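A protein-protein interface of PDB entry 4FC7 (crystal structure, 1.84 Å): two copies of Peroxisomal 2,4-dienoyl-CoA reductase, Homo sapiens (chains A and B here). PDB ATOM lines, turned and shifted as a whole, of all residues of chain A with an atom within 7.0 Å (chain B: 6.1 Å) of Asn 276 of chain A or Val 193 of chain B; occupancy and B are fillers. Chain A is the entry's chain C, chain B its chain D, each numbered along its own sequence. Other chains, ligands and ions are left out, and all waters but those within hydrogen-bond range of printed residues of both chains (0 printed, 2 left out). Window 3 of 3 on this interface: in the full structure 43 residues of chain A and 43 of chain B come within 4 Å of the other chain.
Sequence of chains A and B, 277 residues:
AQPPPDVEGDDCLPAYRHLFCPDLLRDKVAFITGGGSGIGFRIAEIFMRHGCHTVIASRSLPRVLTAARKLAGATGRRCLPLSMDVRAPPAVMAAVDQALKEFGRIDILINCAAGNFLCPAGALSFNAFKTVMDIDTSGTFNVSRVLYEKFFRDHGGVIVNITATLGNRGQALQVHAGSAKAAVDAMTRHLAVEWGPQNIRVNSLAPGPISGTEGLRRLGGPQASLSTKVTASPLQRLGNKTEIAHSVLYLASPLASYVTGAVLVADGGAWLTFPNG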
ATOM      1  N   LEU A 166     -32.727   3.050   0.900  1.00  0.00           N
ATOM      2  CA  LEU A 166     -31.683   3.182   1.986  1.00  0.00           C
ATOM      3  C   LEU A 166     -31.187   4.617   2.151  1.00  0.00           C
ATOM      4  O   LEU A 166     -30.868   5.056   3.297  1.00  0.00           O
ATOM      5  CB  LEU A 166     -30.497   2.336   1.616  1.00  0.00           C
ATOM      6  CG  LEU A 166     -30.793   0.851   1.491  1.00  0.00           C
ATOM      7  CD1 LEU A 166     -29.677   0.304   0.592  1.00  0.00           C
ATOM      8  CD2 LEU A 166     -30.877   0.138   2.899  1.00  0.00           C
ATOM      9  N   ARG A 169     -33.112   7.888   4.617  1.00  0.00           N
ATOM     10  CA  ARG A 169     -32.740   8.186   6.053  1.00  0.00           C
ATOM     11  C   ARG A 169     -31.253   7.925   6.344  1.00  0.00           C
ATOM     12  O   ARG A 169     -30.794   7.979   7.513  1.00  0.00           O
ATOM     13  CB  ARG A 169     -33.606   7.355   7.017  1.00  0.00           C
ATOM     14  CG  ARG A 169     -35.091   7.675   6.915  1.00  0.00           C
ATOM     15  CD  ARG A 169     -36.017   6.647   7.630  1.00  0.00           C
ATOM     16  NE  ARG A 169     -35.545   6.421   9.007  1.00  0.00           N
ATOM     17  CZ  ARG A 169     -35.870   5.337   9.731  1.00  0.00           C
ATOM     18  NH1 ARG A 169     -36.761   4.460   9.237  1.00  0.00           N
ATOM     19  NH2 ARG A 169     -35.310   5.143  10.953  1.00  0.00           N
ATOM     20  N   GLY A 170     -30.502   7.569   5.312  1.00  0.00           N
ATOM     21  CA  GLY A 170     -29.104   7.259   5.539  1.00  0.00           C
ATOM     22  C   GLY A 170     -28.913   6.029   6.413  1.00  0.00           C
ATOM     23  O   GLY A 170     -28.180   6.082   7.436  1.00  0.00           O
ATOM     24  N   GLN A 171     -29.489   4.915   5.988  1.00  0.00           N
ATOM     25  CA  GLN A 171     -29.394   3.661   6.711  1.00  0.00           C
ATOM     26  C   GLN A 171     -27.950   3.303   7.005  1.00  0.00           C
ATOM     27  O   GLN A 171     -27.126   3.228   6.080  1.00  0.00           O
ATOM     28  CB  GLN A 171     -30.016   2.521   5.872  1.00  0.00           C
ATOM     29  CG  GLN A 171     -30.271   1.226   6.606  1.00  0.00           C
ATOM     30  CD  GLN A 171     -31.116   1.456   7.891  1.00  0.00           C
ATOM     31  OE1 GLN A 171     -30.777   0.969   8.986  1.00  0.00           O
ATOM     32  NE2 GLN A 171     -32.207   2.153   7.745  1.00  0.00           N
ATOM     33  N   ALA A 172     -27.653   3.068   8.280  1.00  0.00           N
ATOM     34  CA  ALA A 172     -26.332   2.632   8.779  1.00  0.00           C
ATOM     35  C   ALA A 172     -25.831   1.362   8.101  1.00  0.00           C
ATOM     36  O   ALA A 172     -26.602   0.452   7.803  1.00  0.00           O
ATOM     37  CB  ALA A 172     -26.381   2.414  10.318  1.00  0.00           C
ATOM     38  N   LEU A 173     -24.517   1.307   7.855  1.00  0.00           N
ATOM     39  CA  LEU A 173     -23.842   0.153   7.297  1.00  0.00           C
ATOM     40  C   LEU A 173     -24.076   0.072   5.754  1.00  0.00           C
ATOM     41  O   LEU A 173     -23.668  -0.895   5.140  1.00  0.00           O
ATOM     42  CB  LEU A 173     -24.239  -1.154   7.999  1.00  0.00           C
ATOM     43  CG  LEU A 173     -24.181  -1.252   9.552  1.00  0.00           C
ATOM     44  CD1 LEU A 173     -24.632  -2.636  10.111  1.00  0.00           C
ATOM     45  CD2 LEU A 173     -22.793  -0.871  10.030  1.00  0.00           C
ATOM     46  N   THR A 273     -40.690   3.000   9.155  1.00  0.00           N
ATOM     47  CA  THR A 273     -40.602   2.497  10.542  1.00  0.00           C
ATOM     48  C   THR A 273     -39.305   1.786  10.887  1.00  0.00           C
ATOM     49  O   THR A 273     -39.056   1.623  12.067  1.00  0.00           O
ATOM     50  CB  THR A 273     -41.745   1.539  10.895  1.00  0.00           C
ATOM     51  OG1 THR A 273     -41.606   0.367  10.071  1.00  0.00           O
ATOM     52  CG2 THR A 273     -43.095   2.156  10.667  1.00  0.00           C
ATOM     53  N   PHE A 274     -38.516   1.300   9.903  1.00  0.00           N
ATOM     54  CA  PHE A 274     -37.338   0.447  10.245  1.00  0.00           C
ATOM     55  C   PHE A 274     -36.349   1.258  11.075  1.00  0.00           C
ATOM     56  O   PHE A 274     -36.143   2.447  10.826  1.00  0.00           O
ATOM     57  CB  PHE A 274     -36.634  -0.174   9.003  1.00  0.00           C
ATOM     58  CG  PHE A 274     -37.042  -1.586   8.711  1.00  0.00           C
ATOM     59  CD1 PHE A 274     -38.384  -1.998   8.898  1.00  0.00           C
ATOM     60  CD2 PHE A 274     -36.105  -2.524   8.204  1.00  0.00           C
ATOM     61  CE1 PHE A 274     -38.778  -3.301   8.601  1.00  0.00           C
ATOM     62  CE2 PHE A 274     -36.504  -3.846   7.939  1.00  0.00           C
ATOM     63  CZ  PHE A 274     -37.842  -4.243   8.127  1.00  0.00           C
ATOM     64  N   PRO A 275     -35.708   0.601  12.062  1.00  0.00           N
ATOM     65  CA  PRO A 275     -34.740   1.313  12.921  1.00  0.00           C
ATOM     66  C   PRO A 275     -33.521   1.720  12.118  1.00  0.00           C
ATOM     67  O   PRO A 275     -33.180   1.076  11.098  1.00  0.00           O
ATOM     68  CB  PRO A 275     -34.332   0.256  13.972  1.00  0.00           C
ATOM     69  CG  PRO A 275     -34.765  -1.056  13.446  1.00  0.00           C
ATOM     70  CD  PRO A 275     -35.749  -0.863  12.308  1.00  0.00           C
ATOM     71  N   ASN A 276     -32.851   2.757  12.588  1.00  0.00           N
ATOM     72  CA  ASN A 276     -31.619   3.125  11.971  1.00  0.00           C
ATOM     73  C   ASN A 276     -30.479   3.371  12.964  1.00  0.00           C
ATOM     74  O   ASN A 276     -30.205   4.490  13.404  1.00  0.00           O
ATOM     75  CB  ASN A 276     -31.857   4.296  11.012  1.00  0.00           C
ATOM     76  CG  ASN A 276     -30.615   4.639  10.246  1.00  0.00           C
ATOM     77  OD1 ASN A 276     -29.638   3.888  10.261  1.00  0.00           O
ATOM     78  ND2 ASN A 276     -30.641   5.731   9.590  1.00  0.00           N
ATOM     79  N   THR B 188     -24.412  12.344   2.636  1.00  0.00           N
ATOM     80  CA  THR B 188     -24.536  13.349   3.724  1.00  0.00           C
ATOM     81  C   THR B 188     -25.383  12.740   4.833  1.00  0.00           C
ATOM     82  O   THR B 188     -24.966  12.746   6.029  1.00  0.00           O
ATOM     83  CB  THR B 188     -25.108  14.675   3.225  1.00  0.00           C
ATOM     84  OG1 THR B 188     -24.088  15.337   2.482  1.00  0.00           O
ATOM     85  CG2 THR B 188     -25.558  15.596   4.365  1.00  0.00           C
ATOM     86  N   ARG B 189     -26.534  12.163   4.500  1.00  0.00           N
ATOM     87  CA  ARG B 189     -27.397  11.557   5.517  1.00  0.00           C
ATOM     88  C   ARG B 189     -26.757  10.320   6.168  1.00  0.00           C
ATOM     89  O   ARG B 189     -26.745  10.208   7.333  1.00  0.00           O
ATOM     90  CB  ARG B 189     -28.778  11.261   4.974  1.00  0.00           C
ATOM     91  CG  ARG B 189     -29.557  12.507   4.618  1.00  0.00           C
ATOM     92  CD  ARG B 189     -30.950  12.165   4.177  1.00  0.00           C
ATOM     93  NE  ARG B 189     -30.955  11.526   2.901  1.00  0.00           N
ATOM     94  CZ  ARG B 189     -30.914  12.178   1.753  1.00  0.00           C
ATOM     95  NH1 ARG B 189     -30.935  11.546   0.623  1.00  0.00           N
ATOM     96  NH2 ARG B 189     -30.827  13.479   1.763  1.00  0.00           N
ATOM     97  N   HIS B 190     -26.190   9.446   5.372  1.00  0.00           N
ATOM     98  CA  HIS B 190     -25.536   8.233   5.933  1.00  0.00           C
ATOM     99  C   HIS B 190     -24.385   8.550   6.902  1.00  0.00           C
ATOM    100  O   HIS B 190     -24.286   7.936   7.939  1.00  0.00           O
ATOM    101  CB  HIS B 190     -24.941   7.311   4.838  1.00  0.00           C
ATOM    102  CG  HIS B 190     -25.953   6.577   3.997  1.00  0.00           C
ATOM    103  ND1 HIS B 190     -26.460   5.344   4.342  1.00  0.00           N
ATOM    104  CD2 HIS B 190     -26.432   6.865   2.709  1.00  0.00           C
ATOM    105  CE1 HIS B 190     -27.350   4.921   3.365  1.00  0.00           C
ATOM    106  NE2 HIS B 190     -27.295   5.858   2.341  1.00  0.00           N
ATOM    107  N   LEU B 191     -23.510   9.463   6.526  1.00  0.00           N
ATOM    108  CA  LEU B 191     -22.397   9.866   7.389  1.00  0.00           C
ATOM    109  C   LEU B 191     -22.874  10.630   8.615  1.00  0.00           C
ATOM    110  O   LEU B 191     -22.309  10.468   9.715  1.00  0.00           O
ATOM    111  CB  LEU B 191     -21.328  10.640   6.622  1.00  0.00           C
ATOM    112  CG  LEU B 191     -20.765   9.795   5.442  1.00  0.00           C
ATOM    113  CD1 LEU B 191     -19.730  10.668   4.746  1.00  0.00           C
ATOM    114  CD2 LEU B 191     -20.195   8.439   5.772  1.00  0.00           C
ATOM    115  N   ALA B 192     -23.905  11.441   8.459  1.00  0.00           N
ATOM    116  CA  ALA B 192     -24.444  12.169   9.589  1.00  0.00           C
ATOM    117  C   ALA B 192     -24.887  11.150  10.656  1.00  0.00           C
ATOM    118  O   ALA B 192     -24.643  11.373  11.871  1.00  0.00           O
ATOM    119  CB  ALA B 192     -25.611  13.034   9.180  1.00  0.00           C
ATOM    120  N   VAL B 193     -25.531  10.075  10.203  1.00  0.00           N
ATOM    121  CA  VAL B 193     -26.043   9.057  11.083  1.00  0.00           C
ATOM    122  C   VAL B 193     -24.897   8.234  11.741  1.00  0.00           C
ATOM    123  O   VAL B 193     -24.875   8.112  12.919  1.00  0.00           O
ATOM    124  CB  VAL B 193     -27.040   8.119  10.355  1.00  0.00           C
ATOM    125  CG1 VAL B 193     -27.358   6.879  11.188  1.00  0.00           C
ATOM    126  CG2 VAL B 193     -28.313   8.913  10.074  1.00  0.00           C
ATOM    127  N   GLU B 194     -23.940   7.779  10.960  1.00  0.00           N
ATOM    128  CA  GLU B 194     -22.884   6.962  11.472  1.00  0.00           C
ATOM    129  C   GLU B 194     -21.890   7.729  12.341  1.00  0.00           C
ATOM    130  O   GLU B 194     -21.336   7.173  13.231  1.00  0.00           O
ATOM    131  CB  GLU B 194     -22.146   6.305  10.301  1.00  0.00           C
ATOM    132  CG  GLU B 194     -22.908   5.038   9.879  1.00  0.00           C
ATOM    133  CD  GLU B 194     -22.058   4.037   9.085  1.00  0.00           C
ATOM    134  OE1 GLU B 194     -20.856   3.806   9.418  1.00  0.00           O
ATOM    135  OE2 GLU B 194     -22.596   3.460   8.121  1.00  0.00           O
ATOM    136  N   TRP B 195     -21.626   8.983  11.996  1.00  0.00           N
ATOM    137  CA  TRP B 195     -20.545   9.687  12.588  1.00  0.00           C
ATOM    138  C   TRP B 195     -20.964  10.725  13.571  1.00  0.00           C
ATOM    139  O   TRP B 195     -20.089  11.294  14.246  1.00  0.00           O
ATOM    140  CB  TRP B 195     -19.704  10.340  11.495  1.00  0.00           C
ATOM    141  CG  TRP B 195     -18.977   9.351  10.644  1.00  0.00           C
ATOM    142  CD1 TRP B 195     -18.864   7.984  10.832  1.00  0.00           C
ATOM    143  CD2 TRP B 195     -18.170   9.637   9.456  1.00  0.00           C
ATOM    144  NE1 TRP B 195     -18.089   7.405   9.863  1.00  0.00           N
ATOM    145  CE2 TRP B 195     -17.668   8.341   8.981  1.00  0.00           C
ATOM    146  CE3 TRP B 195     -17.830  10.813   8.745  1.00  0.00           C
ATOM    147  CZ2 TRP B 195     -16.855   8.227   7.816  1.00  0.00           C
ATOM    148  CZ3 TRP B 195     -17.019  10.687   7.586  1.00  0.00           C
ATOM    149  CH2 TRP B 195     -16.514   9.417   7.170  1.00  0.00           C
ATOM    150  N   GLY B 196     -22.273  10.969  13.672  1.00  0.00           N
ATOM    151  CA  GLY B 196     -22.802  11.826  14.721  1.00  0.00           C
ATOM    152  C   GLY B 196     -22.298  11.484  16.136  1.00  0.00           C
ATOM    153  O   GLY B 196     -21.937  12.384  16.900  1.00  0.00           O
ATOM    154  N   PRO B 197     -22.256  10.211  16.474  1.00  0.00           N
ATOM    155  CA  PRO B 197     -21.768   9.854  17.806  1.00  0.00           C
ATOM    156  C   PRO B 197     -20.276  10.102  18.026  1.00  0.00           C
ATOM    157  O   PRO B 197     -19.828   9.992  19.164  1.00  0.00           O
ATOM    158  CB  PRO B 197     -22.095   8.338  17.922  1.00  0.00           C
ATOM    159  CG  PRO B 197     -23.136   8.071  16.864  1.00  0.00           C
ATOM    160  CD  PRO B 197     -22.935   9.087  15.788  1.00  0.00           C
ATOM    161  N   THR B 260     -27.413  18.571  11.365  1.00  0.00           N
ATOM    162  CA  THR B 260     -26.649  17.513  10.789  1.00  0.00           C
ATOM    163  C   THR B 260     -27.611  16.682   9.920  1.00  0.00           C
ATOM    164  O   THR B 260     -28.836  16.529  10.199  1.00  0.00           O
ATOM    165  CB  THR B 260     -25.896  16.652  11.813  1.00  0.00           C
ATOM    166  OG1 THR B 260     -24.932  15.797  11.163  1.00  0.00           O
ATOM    167  CG2 THR B 260     -26.831  15.795  12.634  1.00  0.00           C
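The side-chain carboxylate (OE2) of Glu 194 of chain B sits at hydrogen-bond distance from the backbone NH (N) of Leu 173 of chain A, at 2.9 Å. O of Gln 171 of chain A is in hydrogen-bond range of ND1 of His 190 of chain B, at 2.8 Å.
The side-chain amide oxygen of Gln 171 of chain A lies close to the backbone carbonyl oxygen of Pro 275 of chain A (3.2 Å). O of Arg 169 of chain A lies within hydrogen-bond range of ND2 of Asn 276 of chain A (3.1 Å). O of Phe 274 of chain A is in hydrogen-bond range of NH1 of Arg 169 of chain A. O of Leu 166 of chain A lies within hydrogen-bond range of N of Gln 171 of chain A. The backbone NH of Ala 172 of chain A is in hydrogen-bond range of the side-chain amide oxygen of Asn 276 of chain A, at 2.9 Å. OE1 of Gln 171 of chain A lies close to OD1 of Asn 276 of chain A (3.4 Å).
Among the printed residues, pairs that only touch across the chains: Leu 166 of chain A with His 190 of chain B (3.5 Å), Arg 169 of chain A with Val 193 of chain B (3.7 Å), Gly 170 of chain A with Arg 189 of chain B (3.9 Å), Gly 170 of chain A with His 190 of chain B (3.3 Å), Gly 170 of chain A with Val 193 of chain B (3.7 Å), Ala 172 of chain A with Glu 194 of chain B (3.9 Å) and Asn 276 of chain A with Val 193 of chain B (3.8 Å).
Asn 276 of chain A touches just one residue of chain B: Val 193 (3.8 Å). Val 193 of chain B touches just these residues of chain A: Arg 169, Gly 170 and Asn 276. Printed residues of chain A within 4 Å of Glu 194 of chain B: Ala 172 (3.9 Å) and Leu 173 (2.9 Å). Of the printed residues of chain A, Arg 189 of chain B touches Gly 170 (3.9 Å). Of the printed residues of chain A, His 190 of chain B touches Leu 166, Gly 170 and Gln 171. Of the printed residues of chain B, Ala 172 of chain A touches Glu 194. The nearest printed residue of chain B that does not touch Asn 276 of chain A is Arg 189 of chain B (6.3 Å). The nearest residue of chain A that does not touch Val 193 of chain B is Ala 172 of chain A (4.7 Å). The nearest printed residue of chain A that does not touch Glu 194 of chain B is Gln 171 of chain A (5.0 Å).
Printed residues of chain A that touch a printed residue of chain B: Leu 166, Arg 169, Gly 170, Gln 171, Ala 172, Leu 173 and Asn 276. Hydrophobic or aromatic side chains of chain B within 4 Å of the printed part of chain A: His 190 and Val 193. Among the printed residues, no Asp or Glu carboxylate lies within 4 Å of a Lys or Arg side-chain nitrogen of the other chain.
No position is printed for both chains. Of the 9 pairs that touch across the chains among the printed residues, none has its exchanged pair printed and touching as well.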
